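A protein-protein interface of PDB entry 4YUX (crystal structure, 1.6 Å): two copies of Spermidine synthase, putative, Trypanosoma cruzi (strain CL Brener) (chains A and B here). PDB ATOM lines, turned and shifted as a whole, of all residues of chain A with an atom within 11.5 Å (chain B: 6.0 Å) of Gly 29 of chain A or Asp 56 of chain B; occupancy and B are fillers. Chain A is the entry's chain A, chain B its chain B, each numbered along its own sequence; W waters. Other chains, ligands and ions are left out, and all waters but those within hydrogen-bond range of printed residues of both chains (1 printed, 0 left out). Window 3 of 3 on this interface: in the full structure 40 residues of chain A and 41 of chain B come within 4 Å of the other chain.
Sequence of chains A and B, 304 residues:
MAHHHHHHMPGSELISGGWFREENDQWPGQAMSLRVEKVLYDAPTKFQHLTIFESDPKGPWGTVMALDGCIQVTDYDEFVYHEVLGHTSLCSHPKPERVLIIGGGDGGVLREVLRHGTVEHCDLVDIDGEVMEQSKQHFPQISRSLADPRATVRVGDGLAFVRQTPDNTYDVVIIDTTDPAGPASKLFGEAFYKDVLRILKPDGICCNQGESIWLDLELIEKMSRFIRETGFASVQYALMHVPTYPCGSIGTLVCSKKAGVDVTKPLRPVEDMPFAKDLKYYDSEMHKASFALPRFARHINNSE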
ATOM      1  N   ARG A  21      25.866   8.978 -26.742  1.00  0.00           N
ATOM      2  CA  ARG A  21      25.359   7.765 -26.066  1.00  0.00           C
ATOM      3  C   ARG A  21      23.882   7.858 -25.852  1.00  0.00           C
ATOM      4  O   ARG A  21      23.403   8.720 -25.064  1.00  0.00           O
ATOM      5  CB  ARG A  21      26.063   7.635 -24.699  1.00  0.00           C
ATOM      6  CG  ARG A  21      27.607   7.465 -24.813  1.00  0.00           C
ATOM      7  CD  ARG A  21      28.253   7.256 -23.443  1.00  0.00           C
ATOM      8  NE  ARG A  21      27.748   6.167 -22.557  1.00  0.00           N
ATOM      9  CZ  ARG A  21      27.951   4.835 -22.730  1.00  0.00           C
ATOM     10  NH1 ARG A  21      27.511   3.959 -21.862  1.00  0.00           N
ATOM     11  NH2 ARG A  21      28.507   4.372 -23.793  1.00  0.00           N
ATOM     12  N   GLU A  22      23.149   6.925 -26.431  1.00  0.00           N
ATOM     13  CA  GLU A  22      21.677   7.018 -26.509  1.00  0.00           C
ATOM     14  C   GLU A  22      21.056   6.376 -25.264  1.00  0.00           C
ATOM     15  O   GLU A  22      20.397   5.332 -25.310  1.00  0.00           O
ATOM     16  CB  GLU A  22      21.199   6.430 -27.801  1.00  0.00           C
ATOM     17  CG  GLU A  22      19.749   6.789 -28.104  1.00  0.00           C
ATOM     18  CD  GLU A  22      19.180   6.004 -29.216  1.00  0.00           C
ATOM     19  OE1 GLU A  22      19.458   4.797 -29.318  1.00  0.00           O
ATOM     20  OE2 GLU A  22      18.447   6.556 -30.038  1.00  0.00           O
ATOM     21  N   GLU A  23      21.334   7.047 -24.124  1.00  0.00           N
ATOM     22  CA  GLU A  23      20.828   6.577 -22.801  1.00  0.00           C
ATOM     23  C   GLU A  23      19.442   7.171 -22.621  1.00  0.00           C
ATOM     24  O   GLU A  23      19.234   8.408 -22.756  1.00  0.00           O
ATOM     25  CB  GLU A  23      21.815   6.953 -21.655  1.00  0.00           C
ATOM     26  CG  GLU A  23      23.231   6.428 -21.791  1.00  0.00           C
ATOM     27  CD  GLU A  23      24.139   6.725 -20.601  1.00  0.00           C
ATOM     28  OE1 GLU A  23      23.636   7.230 -19.561  1.00  0.00           O
ATOM     29  OE2 GLU A  23      25.361   6.451 -20.740  1.00  0.00           O
ATOM     30  N   ASN A  24      18.481   6.347 -22.238  1.00  0.00           N
ATOM     31  CA  ASN A  24      17.122   6.765 -22.151  1.00  0.00           C
ATOM     32  C   ASN A  24      16.328   5.872 -21.203  1.00  0.00           C
ATOM     33  O   ASN A  24      16.484   4.663 -21.210  1.00  0.00           O
ATOM     34  CB  ASN A  24      16.502   6.740 -23.543  1.00  0.00           C
ATOM     35  CG  ASN A  24      15.319   7.724 -23.665  1.00  0.00           C
ATOM     36  OD1 ASN A  24      14.200   7.417 -23.207  1.00  0.00           O
ATOM     37  ND2 ASN A  24      15.525   8.822 -24.424  1.00  0.00           N
ATOM     38  N   ASP A  25      15.473   6.509 -20.400  1.00  0.00           N
ATOM     39  CA  ASP A  25      14.511   5.744 -19.548  1.00  0.00           C
ATOM     40  C   ASP A  25      13.522   4.913 -20.284  1.00  0.00           C
ATOM     41  O   ASP A  25      12.933   3.965 -19.688  1.00  0.00           O
ATOM     42  CB  ASP A  25      13.657   6.742 -18.701  1.00  0.00           C
ATOM     43  CG  ASP A  25      14.468   7.505 -17.710  1.00  0.00           C
ATOM     44  OD1 ASP A  25      15.552   7.042 -17.352  1.00  0.00           O
ATOM     45  OD2 ASP A  25      13.956   8.582 -17.316  1.00  0.00           O
ATOM     46  N   GLN A  26      13.402   5.132 -21.610  1.00  0.00           N
ATOM     47  CA  GLN A  26      12.535   4.292 -22.437  1.00  0.00           C
ATOM     48  C   GLN A  26      13.193   2.915 -22.759  1.00  0.00           C
ATOM     49  O   GLN A  26      12.520   1.993 -23.257  1.00  0.00           O
ATOM     50  CB  GLN A  26      12.091   5.001 -23.727  1.00  0.00           C
ATOM     51  CG  GLN A  26      11.121   6.178 -23.455  1.00  0.00           C
ATOM     52  CD  GLN A  26      10.823   6.990 -24.682  1.00  0.00           C
ATOM     53  OE1 GLN A  26       9.664   6.996 -25.192  1.00  0.00           O
ATOM     54  NE2 GLN A  26      11.843   7.726 -25.137  1.00  0.00           N
ATOM     55  N   TRP A  27      14.464   2.807 -22.480  1.00  0.00           N
ATOM     56  CA  TRP A  27      15.174   1.504 -22.654  1.00  0.00           C
ATOM     57  C   TRP A  27      16.295   1.403 -21.632  1.00  0.00           C
ATOM     58  O   TRP A  27      17.477   1.541 -21.906  1.00  0.00           O
ATOM     59  CB  TRP A  27      15.681   1.344 -24.093  1.00  0.00           C
ATOM     60  CG  TRP A  27      16.287   2.583 -24.714  1.00  0.00           C
ATOM     61  CD1 TRP A  27      17.566   3.027 -24.611  1.00  0.00           C
ATOM     62  CD2 TRP A  27      15.577   3.485 -25.555  1.00  0.00           C
ATOM     63  NE1 TRP A  27      17.724   4.184 -25.379  1.00  0.00           N
ATOM     64  CE2 TRP A  27      16.499   4.478 -25.952  1.00  0.00           C
ATOM     65  CE3 TRP A  27      14.296   3.488 -26.093  1.00  0.00           C
ATOM     66  CZ2 TRP A  27      16.120   5.556 -26.779  1.00  0.00           C
ATOM     67  CZ3 TRP A  27      13.892   4.534 -26.885  1.00  0.00           C
ATOM     68  CH2 TRP A  27      14.816   5.569 -27.239  1.00  0.00           C
ATOM     69  N   PRO A  28      15.897   1.161 -20.359  1.00  0.00           N
ATOM     70  CA  PRO A  28      16.848   1.188 -19.297  1.00  0.00           C
ATOM     71  C   PRO A  28      17.928   0.104 -19.445  1.00  0.00           C
ATOM     72  O   PRO A  28      17.678  -1.043 -19.926  1.00  0.00           O
ATOM     73  CB  PRO A  28      16.004   0.877 -18.048  1.00  0.00           C
ATOM     74  CG  PRO A  28      14.595   0.817 -18.448  1.00  0.00           C
ATOM     75  CD  PRO A  28      14.513   0.848 -19.963  1.00  0.00           C
ATOM     76  N   GLY A  29      19.125   0.512 -19.088  1.00  0.00           N
ATOM     77  CA  GLY A  29      20.253  -0.443 -18.990  1.00  0.00           C
ATOM     78  C   GLY A  29      21.005  -0.702 -20.303  1.00  0.00           C
ATOM     79  O   GLY A  29      21.953  -1.532 -20.321  1.00  0.00           O
ATOM     80  N   GLN A  30      20.598  -0.025 -21.363  1.00  0.00           N
ATOM     81  CA  GLN A  30      21.325  -0.174 -22.644  1.00  0.00           C
ATOM     82  C   GLN A  30      21.506   1.137 -23.331  1.00  0.00           C
ATOM     83  O   GLN A  30      20.722   2.095 -23.078  1.00  0.00           O
ATOM     84  CB  GLN A  30      20.506  -1.107 -23.567  1.00  0.00           C
ATOM     85  CG  GLN A  30      19.195  -0.401 -24.063  1.00  0.00           C
ATOM     86  CD  GLN A  30      18.316  -1.429 -24.819  1.00  0.00           C
ATOM     87  OE1 GLN A  30      18.267  -1.421 -26.127  1.00  0.00           O
ATOM     88  NE2 GLN A  30      17.680  -2.320 -24.081  1.00  0.00           N
ATOM     89  N   ALA A  31      22.453   1.186 -24.289  1.00  0.00           N
ATOM     90  CA  ALA A  31      22.629   2.422 -25.063  1.00  0.00           C
ATOM     91  C   ALA A  31      23.470   2.169 -26.270  1.00  0.00           C
ATOM     92  O   ALA A  31      24.626   1.808 -26.133  1.00  0.00           O
ATOM     93  CB  ALA A  31      23.267   3.538 -24.202  1.00  0.00           C
ATOM     94  N   MET A  32      22.889   2.424 -27.446  1.00  0.00           N
ATOM     95  CA  MET A  32      23.630   2.501 -28.648  1.00  0.00           C
ATOM     96  C   MET A  32      24.515   3.787 -28.625  1.00  0.00           C
ATOM     97  O   MET A  32      24.059   4.876 -28.064  1.00  0.00           O
ATOM     98  CB  MET A  32      22.680   2.457 -29.866  1.00  0.00           C
ATOM     99  CG  MET A  32      23.497   2.617 -31.200  1.00  0.00           C
ATOM    100  SD  MET A  32      24.645   1.239 -31.302  1.00  0.00           S
ATOM    101  CE  MET A  32      25.123   1.459 -33.003  1.00  0.00           C
ATOM    102  N   SER A  33      25.757   3.682 -29.033  1.00  0.00           N
ATOM    103  CA  SER A  33      26.628   4.863 -29.123  1.00  0.00           C
ATOM    104  C   SER A  33      27.272   4.980 -30.485  1.00  0.00           C
ATOM    105  O   SER A  33      27.606   4.007 -31.136  1.00  0.00           O
ATOM    106  CB  SER A  33      27.799   4.830 -28.119  1.00  0.00           C
ATOM    107  OG  SER A  33      27.377   4.888 -26.793  1.00  0.00           O
ATOM    108  N   LEU A 215      11.108  -4.170 -26.886  1.00  0.00           N
ATOM    109  CA  LEU A 215      11.042  -3.242 -25.737  1.00  0.00           C
ATOM    110  C   LEU A 215       9.657  -2.796 -25.474  1.00  0.00           C
ATOM    111  O   LEU A 215       9.371  -2.385 -24.299  1.00  0.00           O
ATOM    112  CB  LEU A 215      11.894  -1.971 -25.983  1.00  0.00           C
ATOM    113  CG  LEU A 215      13.419  -2.033 -26.205  1.00  0.00           C
ATOM    114  CD1 LEU A 215      14.121  -0.867 -26.922  1.00  0.00           C
ATOM    115  CD2 LEU A 215      14.218  -2.426 -24.999  1.00  0.00           C
ATOM    116  N   PRO A 246      16.592   1.681 -31.271  1.00  0.00           N
ATOM    117  CA  PRO A 246      16.955   0.756 -30.218  1.00  0.00           C
ATOM    118  C   PRO A 246      16.575  -0.709 -30.442  1.00  0.00           C
ATOM    119  O   PRO A 246      15.414  -0.985 -30.768  1.00  0.00           O
ATOM    120  CB  PRO A 246      16.264   1.345 -28.954  1.00  0.00           C
ATOM    121  CG  PRO A 246      16.240   2.806 -29.272  1.00  0.00           C
ATOM    122  CD  PRO A 246      16.021   2.942 -30.770  1.00  0.00           C
ATOM    123  N   CYS A 247      17.587  -1.581 -30.252  1.00  0.00           N
ATOM    124  CA  CYS A 247      17.565  -3.067 -30.466  1.00  0.00           C
ATOM    125  C   CYS A 247      17.596  -3.443 -31.909  1.00  0.00           C
ATOM    126  O   CYS A 247      17.565  -4.655 -32.210  1.00  0.00           O
ATOM    127  CB  CYS A 247      16.327  -3.780 -29.817  1.00  0.00           C
ATOM    128  SG  CYS A 247      16.336  -3.632 -28.004  1.00  0.00           S
ATOM    129  N   TRP B  19      29.607   0.316 -17.159  1.00  0.00           N
ATOM    130  CA  TRP B  19      29.075  -0.159 -18.445  1.00  0.00           C
ATOM    131  C   TRP B  19      30.070  -1.022 -19.159  1.00  0.00           C
ATOM    132  O   TRP B  19      31.308  -0.853 -19.060  1.00  0.00           O
ATOM    133  CB  TRP B  19      28.844   1.032 -19.383  1.00  0.00           C
ATOM    134  CG  TRP B  19      27.640   1.921 -18.919  1.00  0.00           C
ATOM    135  CD1 TRP B  19      27.620   2.858 -17.856  1.00  0.00           C
ATOM    136  CD2 TRP B  19      26.316   1.930 -19.459  1.00  0.00           C
ATOM    137  NE1 TRP B  19      26.354   3.399 -17.725  1.00  0.00           N
ATOM    138  CE2 TRP B  19      25.559   2.898 -18.735  1.00  0.00           C
ATOM    139  CE3 TRP B  19      25.676   1.231 -20.502  1.00  0.00           C
ATOM    140  CZ2 TRP B  19      24.218   3.160 -19.023  1.00  0.00           C
ATOM    141  CZ3 TRP B  19      24.359   1.514 -20.774  1.00  0.00           C
ATOM    142  CH2 TRP B  19      23.631   2.480 -20.039  1.00  0.00           C
ATOM    143  N   SER B  33      26.232  -0.663 -25.816  1.00  0.00           N
ATOM    144  CA  SER B  33      26.591  -0.508 -24.389  1.00  0.00           C
ATOM    145  C   SER B  33      25.514  -1.198 -23.578  1.00  0.00           C
ATOM    146  O   SER B  33      24.278  -0.985 -23.812  1.00  0.00           O
ATOM    147  CB  SER B  33      26.532   1.047 -23.932  1.00  0.00           C
ATOM    148  OG  SER B  33      27.271   1.893 -24.751  1.00  0.00           O
ATOM    149  N   LEU B  34      25.973  -1.918 -22.516  1.00  0.00           N
ATOM    150  CA  LEU B  34      25.054  -2.515 -21.542  1.00  0.00           C
ATOM    151  C   LEU B  34      25.568  -2.184 -20.140  1.00  0.00           C
ATOM    152  O   LEU B  34      26.781  -2.255 -19.910  1.00  0.00           O
ATOM    153  CB  LEU B  34      25.028  -4.052 -21.725  1.00  0.00           C
ATOM    154  CG  LEU B  34      24.242  -4.436 -22.993  1.00  0.00           C
ATOM    155  CD1 LEU B  34      24.392  -5.985 -23.123  1.00  0.00           C
ATOM    156  CD2 LEU B  34      22.795  -4.047 -23.095  1.00  0.00           C
ATOM    157  N   ARG B  35      24.676  -1.841 -19.256  1.00  0.00           N
ATOM    158  CA  ARG B  35      25.061  -1.528 -17.848  1.00  0.00           C
ATOM    159  C   ARG B  35      25.443  -2.867 -17.193  1.00  0.00           C
ATOM    160  O   ARG B  35      24.857  -3.911 -17.422  1.00  0.00           O
ATOM    161  CB  ARG B  35      23.946  -0.739 -17.133  1.00  0.00           C
ATOM    162  CG  ARG B  35      23.847  -0.995 -15.643  1.00  0.00           C
ATOM    163  CD  ARG B  35      23.750   0.287 -14.806  1.00  0.00           C
ATOM    164  NE  ARG B  35      25.085   0.690 -14.343  1.00  0.00           N
ATOM    165  CZ  ARG B  35      25.770   0.093 -13.360  1.00  0.00           C
ATOM    166  NH1 ARG B  35      25.261  -0.934 -12.688  1.00  0.00           N
ATOM    167  NH2 ARG B  35      26.974   0.535 -13.038  1.00  0.00           N
ATOM    168  N   VAL B  36      26.503  -2.769 -16.422  1.00  0.00           N
ATOM    169  CA  VAL B  36      27.053  -3.945 -15.708  1.00  0.00           C
ATOM    170  C   VAL B  36      26.616  -3.917 -14.215  1.00  0.00           C
ATOM    171  O   VAL B  36      27.028  -2.951 -13.496  1.00  0.00           O
ATOM    172  CB  VAL B  36      28.526  -3.884 -15.740  1.00  0.00           C
ATOM    173  CG1 VAL B  36      29.094  -5.012 -14.864  1.00  0.00           C
ATOM    174  CG2 VAL B  36      29.045  -4.136 -17.189  1.00  0.00           C
ATOM    175  N   GLU B  37      25.825  -4.916 -13.786  1.00  0.00           N
ATOM    176  CA  GLU B  37      25.392  -5.058 -12.357  1.00  0.00           C
ATOM    177  C   GLU B  37      26.515  -5.759 -11.605  1.00  0.00           C
ATOM    178  O   GLU B  37      26.918  -5.330 -10.512  1.00  0.00           O
ATOM    179  CB  GLU B  37      24.028  -5.797 -12.205  1.00  0.00           C
ATOM    180  CG  GLU B  37      23.613  -5.905 -10.715  1.00  0.00           C
ATOM    181  CD  GLU B  37      23.249  -4.512 -10.162  1.00  0.00           C
ATOM    182  OE1 GLU B  37      23.023  -3.538 -10.906  1.00  0.00           O
ATOM    183  OE2 GLU B  37      23.161  -4.390  -8.927  1.00  0.00           O
ATOM    184  N   GLU B  54      26.362  -9.981 -15.138  1.00  0.00           N
ATOM    185  CA  GLU B  54      24.956  -9.765 -14.971  1.00  0.00           C
ATOM    186  C   GLU B  54      24.657  -8.335 -15.325  1.00  0.00           C
ATOM    187  O   GLU B  54      25.282  -7.396 -14.822  1.00  0.00           O
ATOM    188  CB  GLU B  54      24.487 -10.028 -13.507  1.00  0.00           C
ATOM    189  CG  GLU B  54      22.975 -10.154 -13.416  1.00  0.00           C
ATOM    190  CD  GLU B  54      22.429 -11.302 -14.327  1.00  0.00           C
ATOM    191  OE1 GLU B  54      23.125 -12.320 -14.451  1.00  0.00           O
ATOM    192  OE2 GLU B  54      21.305 -11.232 -14.857  1.00  0.00           O
ATOM    193  N   SER B  55      23.762  -8.161 -16.280  1.00  0.00           N
ATOM    194  CA  SER B  55      23.407  -6.793 -16.714  1.00  0.00           C
ATOM    195  C   SER B  55      22.399  -6.124 -15.762  1.00  0.00           C
ATOM    196  O   SER B  55      21.991  -6.734 -14.752  1.00  0.00           O
ATOM    197  CB  SER B  55      22.947  -6.831 -18.175  1.00  0.00           C
ATOM    198  OG  SER B  55      21.625  -7.408 -18.325  1.00  0.00           O
ATOM    199  N   ASP B  56      21.981  -4.902 -16.106  1.00  0.00           N
ATOM    200  CA  ASP B  56      21.086  -4.103 -15.215  1.00  0.00           C
ATOM    201  C   ASP B  56      19.777  -4.843 -14.971  1.00  0.00           C
ATOM    202  O   ASP B  56      19.058  -5.137 -15.925  1.00  0.00           O
ATOM    203  CB  ASP B  56      20.784  -2.770 -15.899  1.00  0.00           C
ATOM    204  CG  ASP B  56      20.163  -1.747 -14.973  1.00  0.00           C
ATOM    205  OD1 ASP B  56      19.565  -2.128 -13.932  1.00  0.00           O
ATOM    206  OD2 ASP B  56      20.217  -0.568 -15.397  1.00  0.00           O
ATOM    207  N   PRO B  57      19.451  -5.158 -13.686  1.00  0.00           N
ATOM    208  CA  PRO B  57      18.152  -5.804 -13.477  1.00  0.00           C
ATOM    209  C   PRO B  57      16.917  -4.977 -13.870  1.00  0.00           C
ATOM    210  O   PRO B  57      15.861  -5.557 -14.024  1.00  0.00           O
ATOM    211  CB  PRO B  57      18.145  -6.142 -11.949  1.00  0.00           C
ATOM    212  CG  PRO B  57      19.342  -5.490 -11.361  1.00  0.00           C
ATOM    213  CD  PRO B  57      20.208  -4.905 -12.434  1.00  0.00           C
ATOM    214  N   LYS B  58      17.059  -3.644 -14.049  1.00  0.00           N
ATOM    215  CA  LYS B  58      15.989  -2.776 -14.578  1.00  0.00           C
ATOM    216  C   LYS B  58      15.776  -2.960 -16.086  1.00  0.00           C
ATOM    217  O   LYS B  58      14.769  -2.498 -16.647  1.00  0.00           O
ATOM    218  CB  LYS B  58      16.263  -1.256 -14.328  1.00  0.00           C
ATOM    219  CG  LYS B  58      16.480  -0.806 -12.874  1.00  0.00           C
ATOM    220  CD  LYS B  58      15.478   0.229 -12.419  1.00  0.00           C
ATOM    221  CE  LYS B  58      15.165   0.097 -10.914  1.00  0.00           C
ATOM    222  NZ  LYS B  58      14.803  -1.298 -10.478  1.00  0.00           N
ATOM    223  N   GLY B  59      16.761  -3.577 -16.747  1.00  0.00           N
ATOM    224  CA  GLY B  59      16.634  -3.893 -18.164  1.00  0.00           C
ATOM    225  C   GLY B  59      16.415  -5.392 -18.350  1.00  0.00           C
ATOM    226  O   GLY B  59      16.419  -6.149 -17.375  1.00  0.00           O
ATOM    227  N   PRO B  60      16.145  -5.845 -19.604  1.00  0.00           N
ATOM    228  CA  PRO B  60      15.625  -7.197 -19.915  1.00  0.00           C
ATOM    229  C   PRO B  60      16.765  -8.239 -20.172  1.00  0.00           C
ATOM    230  O   PRO B  60      16.426  -9.452 -20.326  1.00  0.00           O
ATOM    231  CB  PRO B  60      14.799  -6.923 -21.196  1.00  0.00           C
ATOM    232  CG  PRO B  60      15.722  -5.936 -21.901  1.00  0.00           C
ATOM    233  CD  PRO B  60      16.016  -4.957 -20.796  1.00  0.00           C
ATOM    234  N   TRP B  61      18.044  -7.840 -20.232  1.00  0.00           N
ATOM    235  CA  TRP B  61      19.078  -8.652 -20.901  1.00  0.00           C
ATOM    236  C   TRP B  61      19.593  -9.814 -20.092  1.00  0.00           C
ATOM    237  O   TRP B  61      20.092 -10.822 -20.662  1.00  0.00           O
ATOM    238  CB  TRP B  61      20.271  -7.749 -21.424  1.00  0.00           C
ATOM    239  CG  TRP B  61      19.708  -6.688 -22.348  1.00  0.00           C
ATOM    240  CD1 TRP B  61      19.352  -5.365 -22.050  1.00  0.00           C
ATOM    241  CD2 TRP B  61      19.240  -6.911 -23.702  1.00  0.00           C
ATOM    242  NE1 TRP B  61      18.739  -4.785 -23.154  1.00  0.00           N
ATOM    243  CE2 TRP B  61      18.607  -5.724 -24.149  1.00  0.00           C
ATOM    244  CE3 TRP B  61      19.261  -8.014 -24.553  1.00  0.00           C
ATOM    245  CZ2 TRP B  61      18.065  -5.568 -25.424  1.00  0.00           C
ATOM    246  CZ3 TRP B  61      18.671  -7.890 -25.783  1.00  0.00           C
ATOM    247  CH2 TRP B  61      18.094  -6.673 -26.240  1.00  0.00           C
ATOM    248  N   GLY B  62      19.479  -9.720 -18.772  1.00  0.00           N
ATOM    249  CA  GLY B  62      20.046 -10.820 -18.005  1.00  0.00           C
ATOM    250  C   GLY B  62      21.527 -10.959 -18.031  1.00  0.00           C
ATOM    251  O   GLY B  62      22.324 -10.010 -18.079  1.00  0.00           O
HETATM  252  O   HOH W   1      21.753  -3.809 -18.818  1.00  0.00           O
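NE2 of Gln 30 of chain A lies close to NE1 of Trp 61 of chain B. The backbone NH of Ala 31 of chain A is in hydrogen-bond range of the backbone carbonyl oxygen of Ser 33 of chain B (2.9 Å). The backbone NH of Arg 35 of chain B sits at hydrogen-bond distance from the backbone carbonyl oxygen of Gly 29 of chain A, 2.9 Å away. The guanidinium group (NH2) of Arg 21 of chain A sits at hydrogen-bond distance from the side-chain hydroxyl (OG) of Ser 33 of chain B.
The backbone NH (N) of Lys 58 of chain B lies within hydrogen-bond range of the side-chain carboxylate (OD1) of Asp 56 of chain B (2.9 Å). NH2 of Arg 21 of chain A lies within hydrogen-bond range of OG of Ser 33 of chain A (3.2 Å). The guanidinium group (NE) of Arg 21 of chain A lies within salt-bridge range of the side-chain carboxylate (OE2) of Glu 23 of chain A (3.0 Å). The side-chain sulfur (SG) of Cys 247 of chain A lies within hydrogen-bond range of the side-chain amide oxygen (OE1) of Gln 30 of chain A (3.5 Å). The guanidinium group (NH1) of Arg 35 of chain B lies within salt-bridge range of the side-chain carboxylate (OE1) of Glu 37 of chain B. N of Asp 56 of chain B lies within hydrogen-bond range of O of Arg 35 of chain B (3.3 Å).
Among the printed residues, pairs that only touch across the chains: Arg 21 of chain A with Trp 19 of chain B, Glu 23 of chain A with Trp 19 of chain B, Pro 28 of chain A with Lys 58 of chain B, Pro 28 of chain A with Gly 59 of chain B, Gly 29 of chain A with Trp 19 of chain B, Gly 29 of chain A with Leu 34 of chain B, Gly 29 of chain A with Asp 56 of chain B, Gln 30 of chain A with Trp 19 of chain B, Gln 30 of chain A with Ser 33 of chain B, Gln 30 of chain A with Leu 34 of chain B, Ser 33 of chain A with Ser 33 of chain B and Cys 247 of chain A with Trp 61 of chain B.
Gly 29 of chain A touches just these residues of chain B: Trp 19 (3.9 Å), Leu 34 (3.5 Å), Arg 35 (2.9 Å) and Asp 56 (3.6 Å). Of chain A, only Gly 29 (3.6 Å) comes within 4 Å of Asp 56 of chain B. Leu 34 of chain B touches two residues of chain A. Arg 35 of chain B touches just one residue of chain A: Gly 29 (2.9 Å). No residue of chain A comes within 4 Å of Ser 55 of chain B. No residue of chain A comes within 4 Å of Pro 57 of chain B. Gly 59 of chain B touches just one residue of chain A: Pro 28 (3.5 Å). No residue of chain A comes within 4 Å of Pro 60 of chain B. No residue of chain A comes within 4 Å of Gly 62 of chain B. Printed residues of chain B within 4 Å of Ser 33 of chain A: Ser 33. Of the printed residues of chain B, Cys 247 of chain A touches Trp 61 (3.7 Å). Of the printed residues of chain B, Gln 30 of chain A touches Trp 19 (3.8 Å), Ser 33 (3.3 Å), Leu 34 (3.8 Å) and Trp 61 (2.8 Å). Printed residues of chain B within 4 Å of Arg 21 of chain A: Trp 19 (3.4 Å) and Ser 33 (2.9 Å). Glu 54 of chain B touches none of the printed residues of chain A. Glu 37 of chain B touches none of the printed residues of chain A. The nearest residue of chain B that does not touch Gly 29 of chain A is Ser 33 of chain B (4.2 Å).
Hydrophobic or aromatic side chains of chain A that line the printed part of chain B: Pro 28. Hydrophobic or aromatic side chains of chain B that line the printed part of chain A: Trp 19, Leu 34 and Trp 61. Along chain B the printed residues that touch a printed residue of chain A span positions 19 to 61. Among the printed residues, 16 pairs touch across the chains.
Ser 33 of chain A touches its own counterpart, Ser 33 of chain B. 1 position is printed for both chains.
Water W1 lies within hydrogen-bond range of the backbone carbonyl oxygen of Gly 29 of chain A (2.7 Å), the backbone NH of Asp 56 of chain B (2.9 Å) and the backbone carbonyl oxygen of Arg 35 of chain B (3.4 Å).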
